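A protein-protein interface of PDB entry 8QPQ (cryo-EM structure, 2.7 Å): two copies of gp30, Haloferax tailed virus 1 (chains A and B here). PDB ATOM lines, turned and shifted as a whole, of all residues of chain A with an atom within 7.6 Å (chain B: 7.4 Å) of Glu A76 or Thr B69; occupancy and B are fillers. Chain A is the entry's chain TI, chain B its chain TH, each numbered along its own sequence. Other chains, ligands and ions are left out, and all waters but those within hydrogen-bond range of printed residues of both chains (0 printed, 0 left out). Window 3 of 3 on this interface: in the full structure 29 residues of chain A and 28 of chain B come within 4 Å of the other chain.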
ATOM      1  N   ALA A  44       8.186 -28.002  22.495  1.00  0.00           N
ATOM      2  CA  ALA A  44       8.721 -26.720  22.074  1.00  0.00           C
ATOM      3  C   ALA A  44       8.778 -25.828  23.310  1.00  0.00           C
ATOM      4  O   ALA A  44       7.743 -25.581  23.921  1.00  0.00           O
ATOM      5  CB  ALA A  44       7.822 -26.146  20.986  1.00  0.00           C
ATOM      6  N   NEP A  45       9.956 -25.315  23.696  1.00  0.00           N
ATOM      7  CA  NEP A  45      10.137 -24.972  25.100  1.00  0.00           C
ATOM      8  C   NEP A  45      10.456 -23.503  25.419  1.00  0.00           C
ATOM      9  O   NEP A  45      10.358 -23.137  26.592  1.00  0.00           O
ATOM     10  CB  NEP A  45      11.111 -25.965  25.774  1.00  0.00           C
ATOM     11  CG  NEP A  45      12.410 -26.248  25.078  1.00  0.00           C
ATOM     12  ND1 NEP A  45      13.568 -25.497  25.288  1.00  0.00           N
ATOM     13  CD2 NEP A  45      12.710 -27.275  24.231  1.00  0.00           C
ATOM     14  CE1 NEP A  45      14.506 -26.111  24.595  1.00  0.00           C
ATOM     15  NE2 NEP A  45      14.070 -27.202  23.896  1.00  0.00           N
ATOM     16  P   NEP A  45      15.047 -28.329  22.967  1.00  0.00           P
ATOM     17  O1P NEP A  45      16.408 -28.346  23.668  1.00  0.00           O
ATOM     18  O2P NEP A  45      14.300 -29.600  23.123  1.00  0.00           O
ATOM     19  O3P NEP A  45      15.079 -27.714  21.606  1.00  0.00           O
ATOM     20  N   GLY A  46      10.832 -22.658  24.446  1.00  0.00           N
ATOM     21  CA  GLY A  46      10.944 -21.210  24.686  1.00  0.00           C
ATOM     22  C   GLY A  46      12.115 -20.743  25.568  1.00  0.00           C
ATOM     23  O   GLY A  46      12.557 -19.602  25.447  1.00  0.00           O
ATOM     24  N   GLY A  47      12.648 -21.653  26.395  1.00  0.00           N
ATOM     25  CA  GLY A  47      13.836 -21.502  27.221  1.00  0.00           C
ATOM     26  C   GLY A  47      14.154 -22.852  27.861  1.00  0.00           C
ATOM     27  O   GLY A  47      13.520 -23.824  27.528  1.00  0.00           O
ATOM     28  N   SER A  48      15.140 -22.924  28.751  1.00  0.00           N
ATOM     29  CA  SER A  48      15.591 -24.182  29.336  1.00  0.00           C
ATOM     30  C   SER A  48      14.502 -24.870  30.170  1.00  0.00           C
ATOM     31  O   SER A  48      13.827 -24.227  30.977  1.00  0.00           O
ATOM     32  CB  SER A  48      16.817 -23.964  30.191  1.00  0.00           C
ATOM     33  OG  SER A  48      17.831 -23.332  29.434  1.00  0.00           O
ATOM     34  N   PHE A  73      16.687 -29.787  28.539  1.00  0.00           N
ATOM     35  CA  PHE A  73      16.776 -29.026  27.307  1.00  0.00           C
ATOM     36  C   PHE A  73      17.249 -27.612  27.635  1.00  0.00           C
ATOM     37  O   PHE A  73      16.786 -27.018  28.615  1.00  0.00           O
ATOM     38  CB  PHE A  73      15.363 -28.986  26.727  1.00  0.00           C
ATOM     39  CG  PHE A  73      14.780 -30.295  26.247  1.00  0.00           C
ATOM     40  CD1 PHE A  73      15.572 -31.353  25.819  1.00  0.00           C
ATOM     41  CD2 PHE A  73      13.402 -30.465  26.208  1.00  0.00           C
ATOM     42  CE1 PHE A  73      14.997 -32.547  25.393  1.00  0.00           C
ATOM     43  CE2 PHE A  73      12.822 -31.617  25.696  1.00  0.00           C
ATOM     44  CZ  PHE A  73      13.625 -32.679  25.358  1.00  0.00           C
ATOM     45  N   THR A  74      18.185 -27.075  26.841  1.00  0.00           N
ATOM     46  CA  THR A  74      18.766 -25.759  27.119  1.00  0.00           C
ATOM     47  C   THR A  74      18.434 -24.774  25.999  1.00  0.00           C
ATOM     48  O   THR A  74      18.392 -25.135  24.823  1.00  0.00           O
ATOM     49  CB  THR A  74      20.283 -25.826  27.370  1.00  0.00           C
ATOM     50  OG1 THR A  74      20.939 -26.418  26.249  1.00  0.00           O
ATOM     51  CG2 THR A  74      20.632 -26.619  28.606  1.00  0.00           C
ATOM     52  N   GLY A  75      18.206 -23.511  26.385  1.00  0.00           N
ATOM     53  CA  GLY A  75      17.836 -22.460  25.445  1.00  0.00           C
ATOM     54  C   GLY A  75      16.458 -22.699  24.831  1.00  0.00           C
ATOM     55  O   GLY A  75      15.640 -23.446  25.361  1.00  0.00           O
ATOM     56  N   GLU A  76      16.209 -22.060  23.672  1.00  0.00           N
ATOM     57  CA  GLU A  76      14.931 -22.184  22.990  1.00  0.00           C
ATOM     58  C   GLU A  76      15.053 -23.198  21.843  1.00  0.00           C
ATOM     59  O   GLU A  76      15.999 -23.155  21.050  1.00  0.00           O
ATOM     60  CB  GLU A  76      14.493 -20.798  22.505  1.00  0.00           C
ATOM     61  CG  GLU A  76      13.241 -20.803  21.669  1.00  0.00           C
ATOM     62  CD  GLU A  76      12.636 -19.434  21.415  1.00  0.00           C
ATOM     63  OE1 GLU A  76      13.386 -18.435  21.431  1.00  0.00           O
ATOM     64  OE2 GLU A  76      11.408 -19.365  21.175  1.00  0.00           O
ATOM     65  N   GLY A  77      14.022 -24.037  21.686  1.00  0.00           N
ATOM     66  CA  GLY A  77      13.921 -24.897  20.521  1.00  0.00           C
ATOM     67  C   GLY A  77      12.805 -25.920  20.658  1.00  0.00           C
ATOM     68  O   GLY A  77      11.885 -25.723  21.416  1.00  0.00           O
ATOM     69  N   ILE A  78      12.904 -26.993  19.856  1.00  0.00           N
ATOM     70  CA  ILE A  78      11.951 -28.083  19.878  1.00  0.00           C
ATOM     71  C   ILE A  78      12.658 -29.442  19.900  1.00  0.00           C
ATOM     72  O   ILE A  78      13.456 -29.777  19.004  1.00  0.00           O
ATOM     73  CB  ILE A  78      10.931 -27.981  18.716  1.00  0.00           C
ATOM     74  CG1 ILE A  78       9.859 -29.070  18.804  1.00  0.00           C
ATOM     75  CG2 ILE A  78      11.632 -27.951  17.353  1.00  0.00           C
ATOM     76  CD1 ILE A  78       8.721 -28.891  17.812  1.00  0.00           C
ATOM     77  N   SER A 100      14.979 -21.660  33.277  1.00  0.00           N
ATOM     78  CA  SER A 100      15.561 -20.558  32.509  1.00  0.00           C
ATOM     79  C   SER A 100      16.040 -19.367  33.346  1.00  0.00           C
ATOM     80  O   SER A 100      16.808 -18.546  32.836  1.00  0.00           O
ATOM     81  CB  SER A 100      14.580 -20.053  31.483  1.00  0.00           C
ATOM     82  OG  SER A 100      14.025 -21.126  30.772  1.00  0.00           O
ATOM     83  N   ASP A 105       7.417 -19.834  27.377  1.00  0.00           N
ATOM     84  CA  ASP A 105       6.247 -20.446  26.774  1.00  0.00           C
ATOM     85  C   ASP A 105       6.575 -21.899  26.416  1.00  0.00           C
ATOM     86  O   ASP A 105       7.560 -22.156  25.721  1.00  0.00           O
ATOM     87  CB  ASP A 105       5.787 -19.632  25.559  1.00  0.00           C
ATOM     88  CG  ASP A 105       5.452 -18.173  25.841  1.00  0.00           C
ATOM     89  OD1 ASP A 105       5.144 -17.829  26.998  1.00  0.00           O
ATOM     90  OD2 ASP A 105       5.490 -17.373  24.872  1.00  0.00           O
ATOM     91  N   VAL B  49      14.639 -19.013   6.611  1.00  0.00           N
ATOM     92  CA  VAL B  49      13.374 -18.853   7.324  1.00  0.00           C
ATOM     93  C   VAL B  49      13.508 -19.202   8.805  1.00  0.00           C
ATOM     94  O   VAL B  49      14.324 -20.034   9.195  1.00  0.00           O
ATOM     95  CB  VAL B  49      12.213 -19.669   6.707  1.00  0.00           C
ATOM     96  CG1 VAL B  49      11.836 -19.236   5.311  1.00  0.00           C
ATOM     97  CG2 VAL B  49      12.450 -21.167   6.732  1.00  0.00           C
ATOM     98  N   ASP B  50      12.660 -18.567   9.627  1.00  0.00           N
ATOM     99  CA  ASP B  50      12.423 -18.991  10.998  1.00  0.00           C
ATOM    100  C   ASP B  50      11.066 -19.689  11.068  1.00  0.00           C
ATOM    101  O   ASP B  50      10.065 -19.187  10.552  1.00  0.00           O
ATOM    102  CB  ASP B  50      12.408 -17.816  11.973  1.00  0.00           C
ATOM    103  CG  ASP B  50      13.749 -17.160  12.231  1.00  0.00           C
ATOM    104  OD1 ASP B  50      14.813 -17.778  11.945  1.00  0.00           O
ATOM    105  OD2 ASP B  50      13.730 -16.040  12.770  1.00  0.00           O
ATOM    106  N   VAL B  51      11.031 -20.856  11.719  1.00  0.00           N
ATOM    107  CA  VAL B  51       9.797 -21.583  11.958  1.00  0.00           C
ATOM    108  C   VAL B  51       9.380 -21.355  13.405  1.00  0.00           C
ATOM    109  O   VAL B  51      10.179 -21.429  14.325  1.00  0.00           O
ATOM    110  CB  VAL B  51       9.921 -23.083  11.638  1.00  0.00           C
ATOM    111  CG1 VAL B  51       8.574 -23.783  11.766  1.00  0.00           C
ATOM    112  CG2 VAL B  51      10.481 -23.314  10.244  1.00  0.00           C
ATOM    113  N   GLU B  52       8.095 -21.071  13.594  1.00  0.00           N
ATOM    114  CA  GLU B  52       7.592 -20.630  14.881  1.00  0.00           C
ATOM    115  C   GLU B  52       6.245 -21.295  15.170  1.00  0.00           C
ATOM    116  O   GLU B  52       5.402 -21.397  14.290  1.00  0.00           O
ATOM    117  CB  GLU B  52       7.495 -19.115  14.789  1.00  0.00           C
ATOM    118  CG  GLU B  52       7.167 -18.406  16.078  1.00  0.00           C
ATOM    119  CD  GLU B  52       7.720 -16.998  15.990  1.00  0.00           C
ATOM    120  OE1 GLU B  52       7.084 -16.151  15.295  1.00  0.00           O
ATOM    121  OE2 GLU B  52       8.820 -16.771  16.564  1.00  0.00           O
ATOM    122  N   LEU B  53       6.058 -21.765  16.406  1.00  0.00           N
ATOM    123  CA  LEU B  53       4.827 -22.415  16.821  1.00  0.00           C
ATOM    124  C   LEU B  53       4.109 -21.501  17.806  1.00  0.00           C
ATOM    125  O   LEU B  53       4.702 -21.052  18.782  1.00  0.00           O
ATOM    126  CB  LEU B  53       5.187 -23.761  17.455  1.00  0.00           C
ATOM    127  CG  LEU B  53       4.020 -24.693  17.780  1.00  0.00           C
ATOM    128  CD1 LEU B  53       3.346 -25.191  16.510  1.00  0.00           C
ATOM    129  CD2 LEU B  53       4.506 -25.876  18.594  1.00  0.00           C
ATOM    130  N   ALA B  67       4.400 -18.394  22.130  1.00  0.00           N
ATOM    131  CA  ALA B  67       5.128 -18.447  20.869  1.00  0.00           C
ATOM    132  C   ALA B  67       6.536 -18.990  21.104  1.00  0.00           C
ATOM    133  O   ALA B  67       7.248 -18.491  21.972  1.00  0.00           O
ATOM    134  CB  ALA B  67       5.162 -17.084  20.215  1.00  0.00           C
ATOM    135  N   VAL B  68       6.922 -20.023  20.340  1.00  0.00           N
ATOM    136  CA  VAL B  68       8.257 -20.599  20.424  1.00  0.00           C
ATOM    137  C   VAL B  68       8.866 -20.634  19.026  1.00  0.00           C
ATOM    138  O   VAL B  68       8.281 -21.193  18.102  1.00  0.00           O
ATOM    139  CB  VAL B  68       8.239 -22.004  21.057  1.00  0.00           C
ATOM    140  CG1 VAL B  68       9.627 -22.612  21.126  1.00  0.00           C
ATOM    141  CG2 VAL B  68       7.615 -22.009  22.442  1.00  0.00           C
ATOM    142  N   THR B  69      10.064 -20.053  18.868  1.00  0.00           N
ATOM    143  CA  THR B  69      10.787 -20.202  17.614  1.00  0.00           C
ATOM    144  C   THR B  69      11.442 -21.580  17.613  1.00  0.00           C
ATOM    145  O   THR B  69      12.359 -21.839  18.391  1.00  0.00           O
ATOM    146  CB  THR B  69      11.820 -19.096  17.377  1.00  0.00           C
ATOM    147  OG1 THR B  69      11.250 -17.816  17.649  1.00  0.00           O
ATOM    148  CG2 THR B  69      12.378 -19.123  15.972  1.00  0.00           C
ATOM    149  N   LEU B  70      10.937 -22.462  16.745  1.00  0.00           N
ATOM    150  CA  LEU B  70      11.311 -23.865  16.722  1.00  0.00           C
ATOM    151  C   LEU B  70      12.740 -24.037  16.214  1.00  0.00           C
ATOM    152  O   LEU B  70      13.537 -24.716  16.856  1.00  0.00           O
ATOM    153  CB  LEU B  70      10.334 -24.632  15.827  1.00  0.00           C
ATOM    154  CG  LEU B  70       8.863 -24.612  16.235  1.00  0.00           C
ATOM    155  CD1 LEU B  70       8.105 -25.649  15.426  1.00  0.00           C
ATOM    156  CD2 LEU B  70       8.679 -24.901  17.719  1.00  0.00           C
ATOM    157  N   ASP B  71      13.030 -23.443  15.047  1.00  0.00           N
ATOM    158  CA  ASP B  71      14.313 -23.585  14.375  1.00  0.00           C
ATOM    159  C   ASP B  71      14.455 -22.526  13.281  1.00  0.00           C
ATOM    160  O   ASP B  71      13.470 -21.947  12.821  1.00  0.00           O
ATOM    161  CB  ASP B  71      14.486 -24.992  13.789  1.00  0.00           C
ATOM    162  CG  ASP B  71      15.916 -25.500  13.750  1.00  0.00           C
ATOM    163  OD1 ASP B  71      16.852 -24.694  13.994  1.00  0.00           O
ATOM    164  OD2 ASP B  71      16.095 -26.681  13.398  1.00  0.00           O
ATOM    165  N   SER B  72      15.710 -22.287  12.867  1.00  0.00           N
ATOM    166  CA  SER B  72      16.050 -21.421  11.749  1.00  0.00           C
ATOM    167  C   SER B  72      16.698 -22.267  10.649  1.00  0.00           C
ATOM    168  O   SER B  72      17.638 -23.020  10.892  1.00  0.00           O
ATOM    169  CB  SER B  72      16.955 -20.292  12.166  1.00  0.00           C
ATOM    170  OG  SER B  72      16.347 -19.503  13.164  1.00  0.00           O
ATOM    171  N   ARG B  95       3.997 -20.559  12.016  1.00  0.00           N
ATOM    172  CA  ARG B  95       4.384 -19.426  11.191  1.00  0.00           C
ATOM    173  C   ARG B  95       5.782 -19.694  10.630  1.00  0.00           C
ATOM    174  O   ARG B  95       6.694 -20.054  11.370  1.00  0.00           O
ATOM    175  CB  ARG B  95       4.354 -18.163  12.048  1.00  0.00           C
ATOM    176  CG  ARG B  95       4.715 -16.894  11.285  1.00  0.00           C
ATOM    177  CD  ARG B  95       5.004 -15.737  12.229  1.00  0.00           C
ATOM    178  NE  ARG B  95       3.812 -15.201  12.864  1.00  0.00           N
ATOM    179  CZ  ARG B  95       3.698 -14.733  14.103  1.00  0.00           C
ATOM    180  NH1 ARG B  95       2.539 -14.267  14.513  1.00  0.00           N
ATOM    181  NH2 ARG B  95       4.712 -14.711  14.943  1.00  0.00           N
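Hydrophobic or aromatic side chains of chain A within 4 Å of the printed part of chain B: Ala A44 and Ile A78.
Of the 12 printed residues of chain B, 4 touch a printed residue of chain A.
Among the printed residues, no Asp or Glu carboxylate lies within 4 Å of a Lys or Arg side-chain nitrogen of the other chain.
Of the printed residues of chain B, Ala A44 touches Val B68 and Leu B70.
Of the printed residues of chain B, NEP A45 touches Val B68 (3.7 Å).
Gly A75 touches none of the printed residues of chain B.
Glu A76 touches just these residues of chain B: Val B68 and Thr B69.
Printed residues of chain B within 4 Å of Gly A77: Val B68 (3.9 Å) and Leu B70 (3.7 Å).
Of the printed residues of chain B, Ile A78 touches Leu B70.
Ser A100 touches none of the printed residues of chain B.
Printed residues of chain A within 4 Å of Ala B67: Asp A105 (3.1 Å).
Of chain A, only Glu A76 (2.8 Å) comes within 4 Å of Thr B69.
The nearest residue of chain B that does not touch Glu A76 is Ala B67 (4.3 Å).
The nearest residue of chain A that does not touch Thr B69 is Gly A77 (4.04 Å).
The nearest printed residue of chain A that does not touch Ala B67 is Glu A76 (4.3 Å).
The backbone carbonyl oxygen (O) of Val B51 lies within hydrogen-bond range of the backbone NH (N) of Leu B70.
OG1 of Thr B69 sits at hydrogen-bond distance from OE2 of Glu B52 (2.9 Å).
N of Leu B53 lies within hydrogen-bond range of O of Val B68 (2.9 Å).
N of NEP A45 sits at hydrogen-bond distance from the backbone carbonyl oxygen (O) of Gly A77 (3.0 Å).
O3P of NEP A45 lies within hydrogen-bond range of the backbone NH of Ile A78 (2.9 Å).
Among the printed residues, merely in contact across the chains: Ala A44 with Val B68, Ala A44 with Leu B70, NEP A45 with Val B68, Gly A46 with Val B68, Glu A76 with Val B68, Gly A77 with Val B68, Gly A77 with Leu B70, Ile A78 with Leu B70 and Asp A105 with Val B68.
The backbone NH (N) of Ala B67 sits close to the side-chain carboxylate (OD2) of Asp A105 (3.1 Å).
N of Thr B69 lies within hydrogen-bond range of OE2 of Glu A76 (2.8 Å).
No position is printed for both chains.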
